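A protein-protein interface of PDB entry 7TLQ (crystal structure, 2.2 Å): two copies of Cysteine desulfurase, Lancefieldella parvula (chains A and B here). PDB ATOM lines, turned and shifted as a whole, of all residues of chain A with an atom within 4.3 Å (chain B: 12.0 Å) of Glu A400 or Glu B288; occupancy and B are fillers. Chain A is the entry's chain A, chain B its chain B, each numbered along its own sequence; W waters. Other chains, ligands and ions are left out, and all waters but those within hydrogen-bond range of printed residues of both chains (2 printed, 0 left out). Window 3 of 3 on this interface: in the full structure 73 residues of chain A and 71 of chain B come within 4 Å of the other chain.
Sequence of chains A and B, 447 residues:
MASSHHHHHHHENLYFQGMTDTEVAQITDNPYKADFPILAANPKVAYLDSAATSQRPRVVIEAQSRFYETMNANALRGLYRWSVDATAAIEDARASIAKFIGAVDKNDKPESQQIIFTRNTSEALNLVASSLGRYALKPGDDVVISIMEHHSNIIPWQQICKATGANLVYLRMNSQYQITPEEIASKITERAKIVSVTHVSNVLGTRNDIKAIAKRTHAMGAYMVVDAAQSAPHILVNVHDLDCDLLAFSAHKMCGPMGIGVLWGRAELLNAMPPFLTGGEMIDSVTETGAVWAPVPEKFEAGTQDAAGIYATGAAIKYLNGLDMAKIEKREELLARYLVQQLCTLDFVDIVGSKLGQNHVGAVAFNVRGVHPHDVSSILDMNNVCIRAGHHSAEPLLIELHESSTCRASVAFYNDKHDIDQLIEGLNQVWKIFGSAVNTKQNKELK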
ATOM      1  N   ILE A 147     -29.132  12.629 -25.903  1.00  0.00           N
ATOM      2  CA  ILE A 147     -28.453  11.461 -25.358  1.00  0.00           C
ATOM      3  C   ILE A 147     -29.431  10.364 -24.962  1.00  0.00           C
ATOM      4  O   ILE A 147     -29.015   9.220 -24.748  1.00  0.00           O
ATOM      5  CB  ILE A 147     -27.571  11.892 -24.167  1.00  0.00           C
ATOM      6  CG1 ILE A 147     -26.598  10.782 -23.757  1.00  0.00           C
ATOM      7  CG2 ILE A 147     -28.431  12.321 -22.992  1.00  0.00           C
ATOM      8  CD1 ILE A 147     -25.696  10.309 -24.876  1.00  0.00           C
ATOM      9  N   GLN A 158     -26.000   8.775 -37.601  1.00  0.00           N
ATOM     10  CA  GLN A 158     -24.580   8.489 -37.792  1.00  0.00           C
ATOM     11  C   GLN A 158     -24.279   8.228 -39.262  1.00  0.00           C
ATOM     12  O   GLN A 158     -23.292   8.735 -39.808  1.00  0.00           O
ATOM     13  CB  GLN A 158     -24.159   7.286 -36.950  1.00  0.00           C
ATOM     14  CG  GLN A 158     -24.161   7.507 -35.451  1.00  0.00           C
ATOM     15  CD  GLN A 158     -23.807   6.242 -34.692  1.00  0.00           C
ATOM     16  OE1 GLN A 158     -23.728   5.159 -35.273  1.00  0.00           O
ATOM     17  NE2 GLN A 158     -23.591   6.373 -33.390  1.00  0.00           N
ATOM     18  N   LEU A 168     -22.934  15.341 -36.040  1.00  0.00           N
ATOM     19  CA  LEU A 168     -23.942  14.786 -35.142  1.00  0.00           C
ATOM     20  C   LEU A 168     -23.736  15.387 -33.755  1.00  0.00           C
ATOM     21  O   LEU A 168     -22.718  15.129 -33.104  1.00  0.00           O
ATOM     22  CB  LEU A 168     -23.851  13.262 -35.104  1.00  0.00           C
ATOM     23  CG  LEU A 168     -24.859  12.537 -34.210  1.00  0.00           C
ATOM     24  CD1 LEU A 168     -26.283  12.866 -34.632  1.00  0.00           C
ATOM     25  CD2 LEU A 168     -24.619  11.036 -34.242  1.00  0.00           C
ATOM     26  N   TYR A 170     -25.245  16.234 -29.784  1.00  0.00           N
ATOM     27  CA  TYR A 170     -26.026  15.569 -28.749  1.00  0.00           C
ATOM     28  C   TYR A 170     -26.512  16.578 -27.717  1.00  0.00           C
ATOM     29  O   TYR A 170     -25.722  17.379 -27.208  1.00  0.00           O
ATOM     30  CB  TYR A 170     -25.201  14.482 -28.053  1.00  0.00           C
ATOM     31  CG  TYR A 170     -25.211  13.152 -28.763  1.00  0.00           C
ATOM     32  CD1 TYR A 170     -24.261  12.853 -29.731  1.00  0.00           C
ATOM     33  CD2 TYR A 170     -26.167  12.190 -28.464  1.00  0.00           C
ATOM     34  CE1 TYR A 170     -24.265  11.636 -30.383  1.00  0.00           C
ATOM     35  CE2 TYR A 170     -26.180  10.970 -29.111  1.00  0.00           C
ATOM     36  CZ  TYR A 170     -25.226  10.698 -30.069  1.00  0.00           C
ATOM     37  OH  TYR A 170     -25.233   9.485 -30.717  1.00  0.00           O
ATOM     38  N   ARG A 172     -27.523  17.036 -23.996  1.00  0.00           N
ATOM     39  CA  ARG A 172     -27.209  16.357 -22.749  1.00  0.00           C
ATOM     40  C   ARG A 172     -28.234  16.708 -21.675  1.00  0.00           C
ATOM     41  O   ARG A 172     -29.034  17.636 -21.818  1.00  0.00           O
ATOM     42  CB  ARG A 172     -25.795  16.720 -22.286  1.00  0.00           C
ATOM     43  CG  ARG A 172     -24.739  16.634 -23.380  1.00  0.00           C
ATOM     44  CD  ARG A 172     -24.267  15.203 -23.585  1.00  0.00           C
ATOM     45  NE  ARG A 172     -23.289  15.094 -24.665  1.00  0.00           N
ATOM     46  CZ  ARG A 172     -22.635  13.977 -24.969  1.00  0.00           C
ATOM     47  NH1 ARG A 172     -22.852  12.871 -24.273  1.00  0.00           N
ATOM     48  NH2 ARG A 172     -21.762  13.968 -25.967  1.00  0.00           N
ATOM     49  N   PRO A 396     -25.909   4.332 -25.692  1.00  0.00           N
ATOM     50  CA  PRO A 396     -25.239   5.619 -25.430  1.00  0.00           C
ATOM     51  C   PRO A 396     -25.769   6.337 -24.202  1.00  0.00           C
ATOM     52  O   PRO A 396     -24.998   7.018 -23.514  1.00  0.00           O
ATOM     53  CB  PRO A 396     -25.510   6.420 -26.708  1.00  0.00           C
ATOM     54  CG  PRO A 396     -25.634   5.395 -27.752  1.00  0.00           C
ATOM     55  CD  PRO A 396     -26.339   4.239 -27.100  1.00  0.00           C
ATOM     56  N   LEU A 397     -27.065   6.212 -23.910  1.00  0.00           N
ATOM     57  CA  LEU A 397     -27.606   6.808 -22.695  1.00  0.00           C
ATOM     58  C   LEU A 397     -27.030   6.136 -21.455  1.00  0.00           C
ATOM     59  O   LEU A 397     -26.639   6.809 -20.495  1.00  0.00           O
ATOM     60  CB  LEU A 397     -29.131   6.711 -22.694  1.00  0.00           C
ATOM     61  CG  LEU A 397     -29.788   6.987 -21.341  1.00  0.00           C
ATOM     62  CD1 LEU A 397     -29.627   8.451 -20.964  1.00  0.00           C
ATOM     63  CD2 LEU A 397     -31.252   6.582 -21.349  1.00  0.00           C
ATOM     64  N   LEU A 398     -26.967   4.803 -21.465  1.00  0.00           N
ATOM     65  CA  LEU A 398     -26.464   4.074 -20.305  1.00  0.00           C
ATOM     66  C   LEU A 398     -24.992   4.376 -20.059  1.00  0.00           C
ATOM     67  O   LEU A 398     -24.556   4.485 -18.908  1.00  0.00           O
ATOM     68  CB  LEU A 398     -26.685   2.574 -20.497  1.00  0.00           C
ATOM     69  CG  LEU A 398     -27.961   1.974 -19.898  1.00  0.00           C
ATOM     70  CD1 LEU A 398     -29.201   2.684 -20.418  1.00  0.00           C
ATOM     71  CD2 LEU A 398     -28.036   0.487 -20.201  1.00  0.00           C
ATOM     72  N   ILE A 399     -24.211   4.513 -21.134  1.00  0.00           N
ATOM     73  CA  ILE A 399     -22.806   4.891 -20.996  1.00  0.00           C
ATOM     74  C   ILE A 399     -22.693   6.279 -20.377  1.00  0.00           C
ATOM     75  O   ILE A 399     -21.821   6.536 -19.537  1.00  0.00           O
ATOM     76  CB  ILE A 399     -22.105   4.819 -22.365  1.00  0.00           C
ATOM     77  CG1 ILE A 399     -22.037   3.371 -22.853  1.00  0.00           C
ATOM     78  CG2 ILE A 399     -20.710   5.421 -22.292  1.00  0.00           C
ATOM     79  CD1 ILE A 399     -21.521   3.228 -24.267  1.00  0.00           C
ATOM     80  N   GLU A 400     -23.581   7.192 -20.780  1.00  0.00           N
ATOM     81  CA  GLU A 400     -23.613   8.531 -20.198  1.00  0.00           C
ATOM     82  C   GLU A 400     -23.869   8.475 -18.696  1.00  0.00           C
ATOM     83  O   GLU A 400     -23.315   9.277 -17.934  1.00  0.00           O
ATOM     84  CB  GLU A 400     -24.689   9.366 -20.897  1.00  0.00           C
ATOM     85  CG  GLU A 400     -24.686  10.872 -20.618  1.00  0.00           C
ATOM     86  CD  GLU A 400     -23.495  11.617 -21.207  1.00  0.00           C
ATOM     87  OE1 GLU A 400     -22.573  10.975 -21.753  1.00  0.00           O
ATOM     88  OE2 GLU A 400     -23.497  12.864 -21.140  1.00  0.00           O
ATOM     89  N   LEU A 401     -24.700   7.533 -18.252  1.00  0.00           N
ATOM     90  CA  LEU A 401     -25.073   7.398 -16.849  1.00  0.00           C
ATOM     91  C   LEU A 401     -24.207   6.398 -16.089  1.00  0.00           C
ATOM     92  O   LEU A 401     -24.514   6.094 -14.930  1.00  0.00           O
ATOM     93  CB  LEU A 401     -26.544   6.989 -16.731  1.00  0.00           C
ATOM     94  CG  LEU A 401     -27.593   7.948 -17.295  1.00  0.00           C
ATOM     95  CD1 LEU A 401     -28.946   7.262 -17.374  1.00  0.00           C
ATOM     96  CD2 LEU A 401     -27.674   9.198 -16.434  1.00  0.00           C
ATOM     97  N   HIS A 402     -23.147   5.881 -16.713  1.00  0.00           N
ATOM     98  CA  HIS A 402     -22.216   4.949 -16.070  1.00  0.00           C
ATOM     99  C   HIS A 402     -22.913   3.657 -15.650  1.00  0.00           C
ATOM    100  O   HIS A 402     -22.698   3.141 -14.551  1.00  0.00           O
ATOM    101  CB  HIS A 402     -21.513   5.598 -14.876  1.00  0.00           C
ATOM    102  CG  HIS A 402     -20.550   6.679 -15.256  1.00  0.00           C
ATOM    103  ND1 HIS A 402     -20.918   8.004 -15.352  1.00  0.00           N
ATOM    104  CD2 HIS A 402     -19.232   6.631 -15.563  1.00  0.00           C
ATOM    105  CE1 HIS A 402     -19.869   8.726 -15.703  1.00  0.00           C
ATOM    106  NE2 HIS A 402     -18.833   7.917 -15.837  1.00  0.00           N
ATOM    107  N   THR B 278     -30.776   0.745 -40.351  1.00  0.00           N
ATOM    108  CA  THR B 278     -29.985   0.747 -39.131  1.00  0.00           C
ATOM    109  C   THR B 278     -30.846   1.184 -37.954  1.00  0.00           C
ATOM    110  O   THR B 278     -31.831   1.910 -38.119  1.00  0.00           O
ATOM    111  CB  THR B 278     -28.770   1.677 -39.249  1.00  0.00           C
ATOM    112  OG1 THR B 278     -29.213   3.032 -39.396  1.00  0.00           O
ATOM    113  CG2 THR B 278     -27.913   1.293 -40.448  1.00  0.00           C
ATOM    114  N   GLY B 279     -30.467   0.739 -36.773  1.00  0.00           N
ATOM    115  CA  GLY B 279     -31.192   1.084 -35.570  1.00  0.00           C
ATOM    116  C   GLY B 279     -31.168  -0.073 -34.586  1.00  0.00           C
ATOM    117  O   GLY B 279     -30.205  -0.837 -34.536  1.00  0.00           O
ATOM    118  N   ILE B 283     -27.875  -4.478 -34.176  1.00  0.00           N
ATOM    119  CA  ILE B 283     -26.549  -4.047 -33.757  1.00  0.00           C
ATOM    120  C   ILE B 283     -25.952  -5.098 -32.847  1.00  0.00           C
ATOM    121  O   ILE B 283     -26.634  -6.007 -32.380  1.00  0.00           O
ATOM    122  CB  ILE B 283     -26.590  -2.709 -33.016  1.00  0.00           C
ATOM    123  CG1 ILE B 283     -27.471  -2.910 -31.784  1.00  0.00           C
ATOM    124  CG2 ILE B 283     -27.086  -1.624 -33.932  1.00  0.00           C
ATOM    125  CD1 ILE B 283     -27.243  -1.962 -30.697  1.00  0.00           C
ATOM    126  N   ASP B 284     -24.676  -4.928 -32.530  1.00  0.00           N
ATOM    127  CA  ASP B 284     -24.181  -5.709 -31.415  1.00  0.00           C
ATOM    128  C   ASP B 284     -23.827  -4.816 -30.234  1.00  0.00           C
ATOM    129  O   ASP B 284     -23.956  -5.244 -29.080  1.00  0.00           O
ATOM    130  CB  ASP B 284     -22.967  -6.531 -31.839  1.00  0.00           C
ATOM    131  CG  ASP B 284     -22.628  -7.597 -30.828  1.00  0.00           C
ATOM    132  OD1 ASP B 284     -23.415  -8.583 -30.832  1.00  0.00           O
ATOM    133  OD2 ASP B 284     -21.655  -7.465 -30.074  1.00  0.00           O
ATOM    134  N   SER B 285     -23.437  -3.566 -30.517  1.00  0.00           N
ATOM    135  CA  SER B 285     -23.137  -2.508 -29.557  1.00  0.00           C
ATOM    136  C   SER B 285     -23.224  -1.167 -30.283  1.00  0.00           C
ATOM    137  O   SER B 285     -23.055  -1.093 -31.503  1.00  0.00           O
ATOM    138  CB  SER B 285     -21.748  -2.688 -28.946  1.00  0.00           C
ATOM    139  OG  SER B 285     -20.752  -2.501 -29.939  1.00  0.00           O
ATOM    140  N   VAL B 286     -23.470  -0.104 -29.510  1.00  0.00           N
ATOM    141  CA  VAL B 286     -23.600   1.264 -30.021  1.00  0.00           C
ATOM    142  C   VAL B 286     -22.875   2.239 -29.099  1.00  0.00           C
ATOM    143  O   VAL B 286     -22.947   2.122 -27.871  1.00  0.00           O
ATOM    144  CB  VAL B 286     -25.081   1.687 -30.168  1.00  0.00           C
ATOM    145  CG1 VAL B 286     -25.193   3.172 -30.464  1.00  0.00           C
ATOM    146  CG2 VAL B 286     -25.718   0.954 -31.307  1.00  0.00           C
ATOM    147  N   THR B 287     -22.185   3.213 -29.698  1.00  0.00           N
ATOM    148  CA  THR B 287     -21.655   4.393 -29.017  1.00  0.00           C
ATOM    149  C   THR B 287     -22.299   5.648 -29.609  1.00  0.00           C
ATOM    150  O   THR B 287     -23.120   5.577 -30.527  1.00  0.00           O
ATOM    151  CB  THR B 287     -20.129   4.467 -29.130  1.00  0.00           C
ATOM    152  OG1 THR B 287     -19.757   4.693 -30.495  1.00  0.00           O
ATOM    153  CG2 THR B 287     -19.492   3.175 -28.641  1.00  0.00           C
ATOM    154  N   GLU B 288     -21.913   6.813 -29.078  1.00  0.00           N
ATOM    155  CA  GLU B 288     -22.465   8.071 -29.576  1.00  0.00           C
ATOM    156  C   GLU B 288     -22.147   8.287 -31.050  1.00  0.00           C
ATOM    157  O   GLU B 288     -22.951   8.883 -31.777  1.00  0.00           O
ATOM    158  CB  GLU B 288     -21.937   9.248 -28.753  1.00  0.00           C
ATOM    159  CG  GLU B 288     -22.706   9.522 -27.472  1.00  0.00           C
ATOM    160  CD  GLU B 288     -22.110  10.664 -26.669  1.00  0.00           C
ATOM    161  OE1 GLU B 288     -21.563  11.605 -27.283  1.00  0.00           O
ATOM    162  OE2 GLU B 288     -22.191  10.623 -25.425  1.00  0.00           O
ATOM    163  N   THR B 289     -20.993   7.804 -31.512  1.00  0.00           N
ATOM    164  CA  THR B 289     -20.510   8.108 -32.851  1.00  0.00           C
ATOM    165  C   THR B 289     -20.478   6.916 -33.795  1.00  0.00           C
ATOM    166  O   THR B 289     -20.377   7.119 -35.009  1.00  0.00           O
ATOM    167  CB  THR B 289     -19.101   8.715 -32.777  1.00  0.00           C
ATOM    168  OG1 THR B 289     -18.218   7.795 -32.121  1.00  0.00           O
ATOM    169  CG2 THR B 289     -19.126  10.023 -32.000  1.00  0.00           C
ATOM    170  N   GLY B 290     -20.560   5.689 -33.283  1.00  0.00           N
ATOM    171  CA  GLY B 290     -20.509   4.521 -34.142  1.00  0.00           C
ATOM    172  C   GLY B 290     -21.329   3.351 -33.639  1.00  0.00           C
ATOM    173  O   GLY B 290     -22.036   3.469 -32.634  1.00  0.00           O
ATOM    174  N   ALA B 291     -21.243   2.216 -34.330  1.00  0.00           N
ATOM    175  CA  ALA B 291     -21.980   1.025 -33.932  1.00  0.00           C
ATOM    176  C   ALA B 291     -21.341  -0.198 -34.571  1.00  0.00           C
ATOM    177  O   ALA B 291     -20.791  -0.123 -35.674  1.00  0.00           O
ATOM    178  CB  ALA B 291     -23.458   1.120 -34.328  1.00  0.00           C
ATOM    179  N   VAL B 292     -21.424  -1.323 -33.865  1.00  0.00           N
ATOM    180  CA  VAL B 292     -20.961  -2.616 -34.356  1.00  0.00           C
ATOM    181  C   VAL B 292     -22.185  -3.453 -34.695  1.00  0.00           C
ATOM    182  O   VAL B 292     -23.089  -3.608 -33.865  1.00  0.00           O
ATOM    183  CB  VAL B 292     -20.070  -3.328 -33.324  1.00  0.00           C
ATOM    184  CG1 VAL B 292     -19.556  -4.644 -33.880  1.00  0.00           C
ATOM    185  CG2 VAL B 292     -18.914  -2.427 -32.911  1.00  0.00           C
ATOM    186  N   TRP B 293     -22.215  -3.991 -35.911  1.00  0.00           N
ATOM    187  CA  TRP B 293     -23.408  -4.675 -36.395  1.00  0.00           C
ATOM    188  C   TRP B 293     -23.556  -6.065 -35.784  1.00  0.00           C
ATOM    189  O   TRP B 293     -22.574  -6.741 -35.476  1.00  0.00           O
ATOM    190  CB  TRP B 293     -23.384  -4.799 -37.921  1.00  0.00           C
ATOM    191  CG  TRP B 293     -23.006  -3.550 -38.659  1.00  0.00           C
ATOM    192  CD1 TRP B 293     -22.071  -3.438 -39.647  1.00  0.00           C
ATOM    193  CD2 TRP B 293     -23.567  -2.239 -38.490  1.00  0.00           C
ATOM    194  NE1 TRP B 293     -22.008  -2.142 -40.097  1.00  0.00           N
ATOM    195  CE2 TRP B 293     -22.916  -1.386 -39.404  1.00  0.00           C
ATOM    196  CE3 TRP B 293     -24.552  -1.704 -37.652  1.00  0.00           C
ATOM    197  CZ2 TRP B 293     -23.216  -0.030 -39.502  1.00  0.00           C
ATOM    198  CZ3 TRP B 293     -24.848  -0.359 -37.752  1.00  0.00           C
ATOM    199  CH2 TRP B 293     -24.183   0.462 -38.671  1.00  0.00           C
HETATM  200  O   HOH W   1     -19.554  11.615 -25.245  1.00  0.00           O
HETATM  201  O   HOH W   2     -22.321   7.937 -24.404  1.00  0.00           O
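The backbone NH (N) of Gly B290 sits close to the side-chain amide nitrogen (NE2) of Gln A158 (3.1 Å).
The side-chain amide nitrogen of Gln A158 is in hydrogen-bond range of the backbone carbonyl oxygen of Glu B288 (3.1 Å).
The backbone carbonyl oxygen (O) of Thr B287 lies within hydrogen-bond range of the side-chain amide nitrogen (NE2) of Gln A158, at 3.0 Å.
O of Glu B288 sits at hydrogen-bond distance from OH of Tyr A170 (2.6 Å).
OE2 of Glu B288 is in salt-bridge range of NH1 of Arg A172.
The side-chain hydroxyl (OG1) of Thr B287 sits close to the backbone NH (N) of Thr B289, at 3.5 Å.
The backbone NH (N) of Gly B290 sits at hydrogen-bond distance from the side-chain hydroxyl (OG1) of Thr B287.
The guanidinium group (NH1) of Arg A172 is in salt-bridge range of the side-chain carboxylate (OE1) of Glu A400, at 3.2 Å.
Among the printed residues, merely in contact across the chains: Ile A147 with Glu B288, Gln A158 with Thr B289, Gln A158 with Ala B291, Leu A168 with Glu B288, Pro A396 with Val B286, Pro A396 with Thr B287 and Glu A400 with Glu B288.
Tyr A170 touches one residue of chain B.
Arg A172 touches just one residue of chain B: Glu B288.
Printed residues of chain B within 4 Å of Pro A396: Val B286 (3.5 Å) and Thr B287 (3.7 Å).
No residue of chain B comes within 4 Å of Leu A397.
Of chain B, only Glu B288 comes within 4 Å of Glu A400.
No residue of chain B comes within 4 Å of Leu A401.
Of the printed residues of chain A, Val B286 touches Pro A396.
Of chain A, only Ile A147, Gln A158, Leu A168, Tyr A170, Arg A172 and Glu A400 come within 4 Å of Glu B288.
Printed residues of chain A within 4 Å of Thr B289: Gln A158.
The nearest printed residue of chain A that does not touch Thr B289 is Tyr A170 (4.6 Å).
Hydrophobic or aromatic side chains of chain B that line the printed part of chain A: Val B286.
Of the 12 printed residues of chain A, 7 touch a printed residue of chain B.
Printed residues of chain A that touch a printed residue of chain B: Ile A147, Gln A158, Leu A168, Tyr A170, Arg A172, Pro A396 and Glu A400.
Hydrophobic or aromatic side chains of chain A that line the printed part of chain B: Ile A147, Leu A168, Tyr A170 and Pro A396.
Among the printed residues, 12 pairs touch across the chains.
Among the printed residues, Asp or Glu carboxylates within 4 Å of a Lys or Arg side-chain nitrogen of the other chain: Arg A172 with Glu B288 (2.6 Å).
No position is printed for both chains.
Of the 12 pairs that touch across the chains among the printed residues, none has its exchanged pair printed and touching as well.
Water W1 lies within hydrogen-bond range of OE2 of Glu B288 and NH2 of Arg A172.
Water W2 bridges the side-chain carboxylate (OE2) of Glu B288 (2.9 Å) and the backbone carbonyl oxygen (O) of Pro A396 (3.0 Å).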
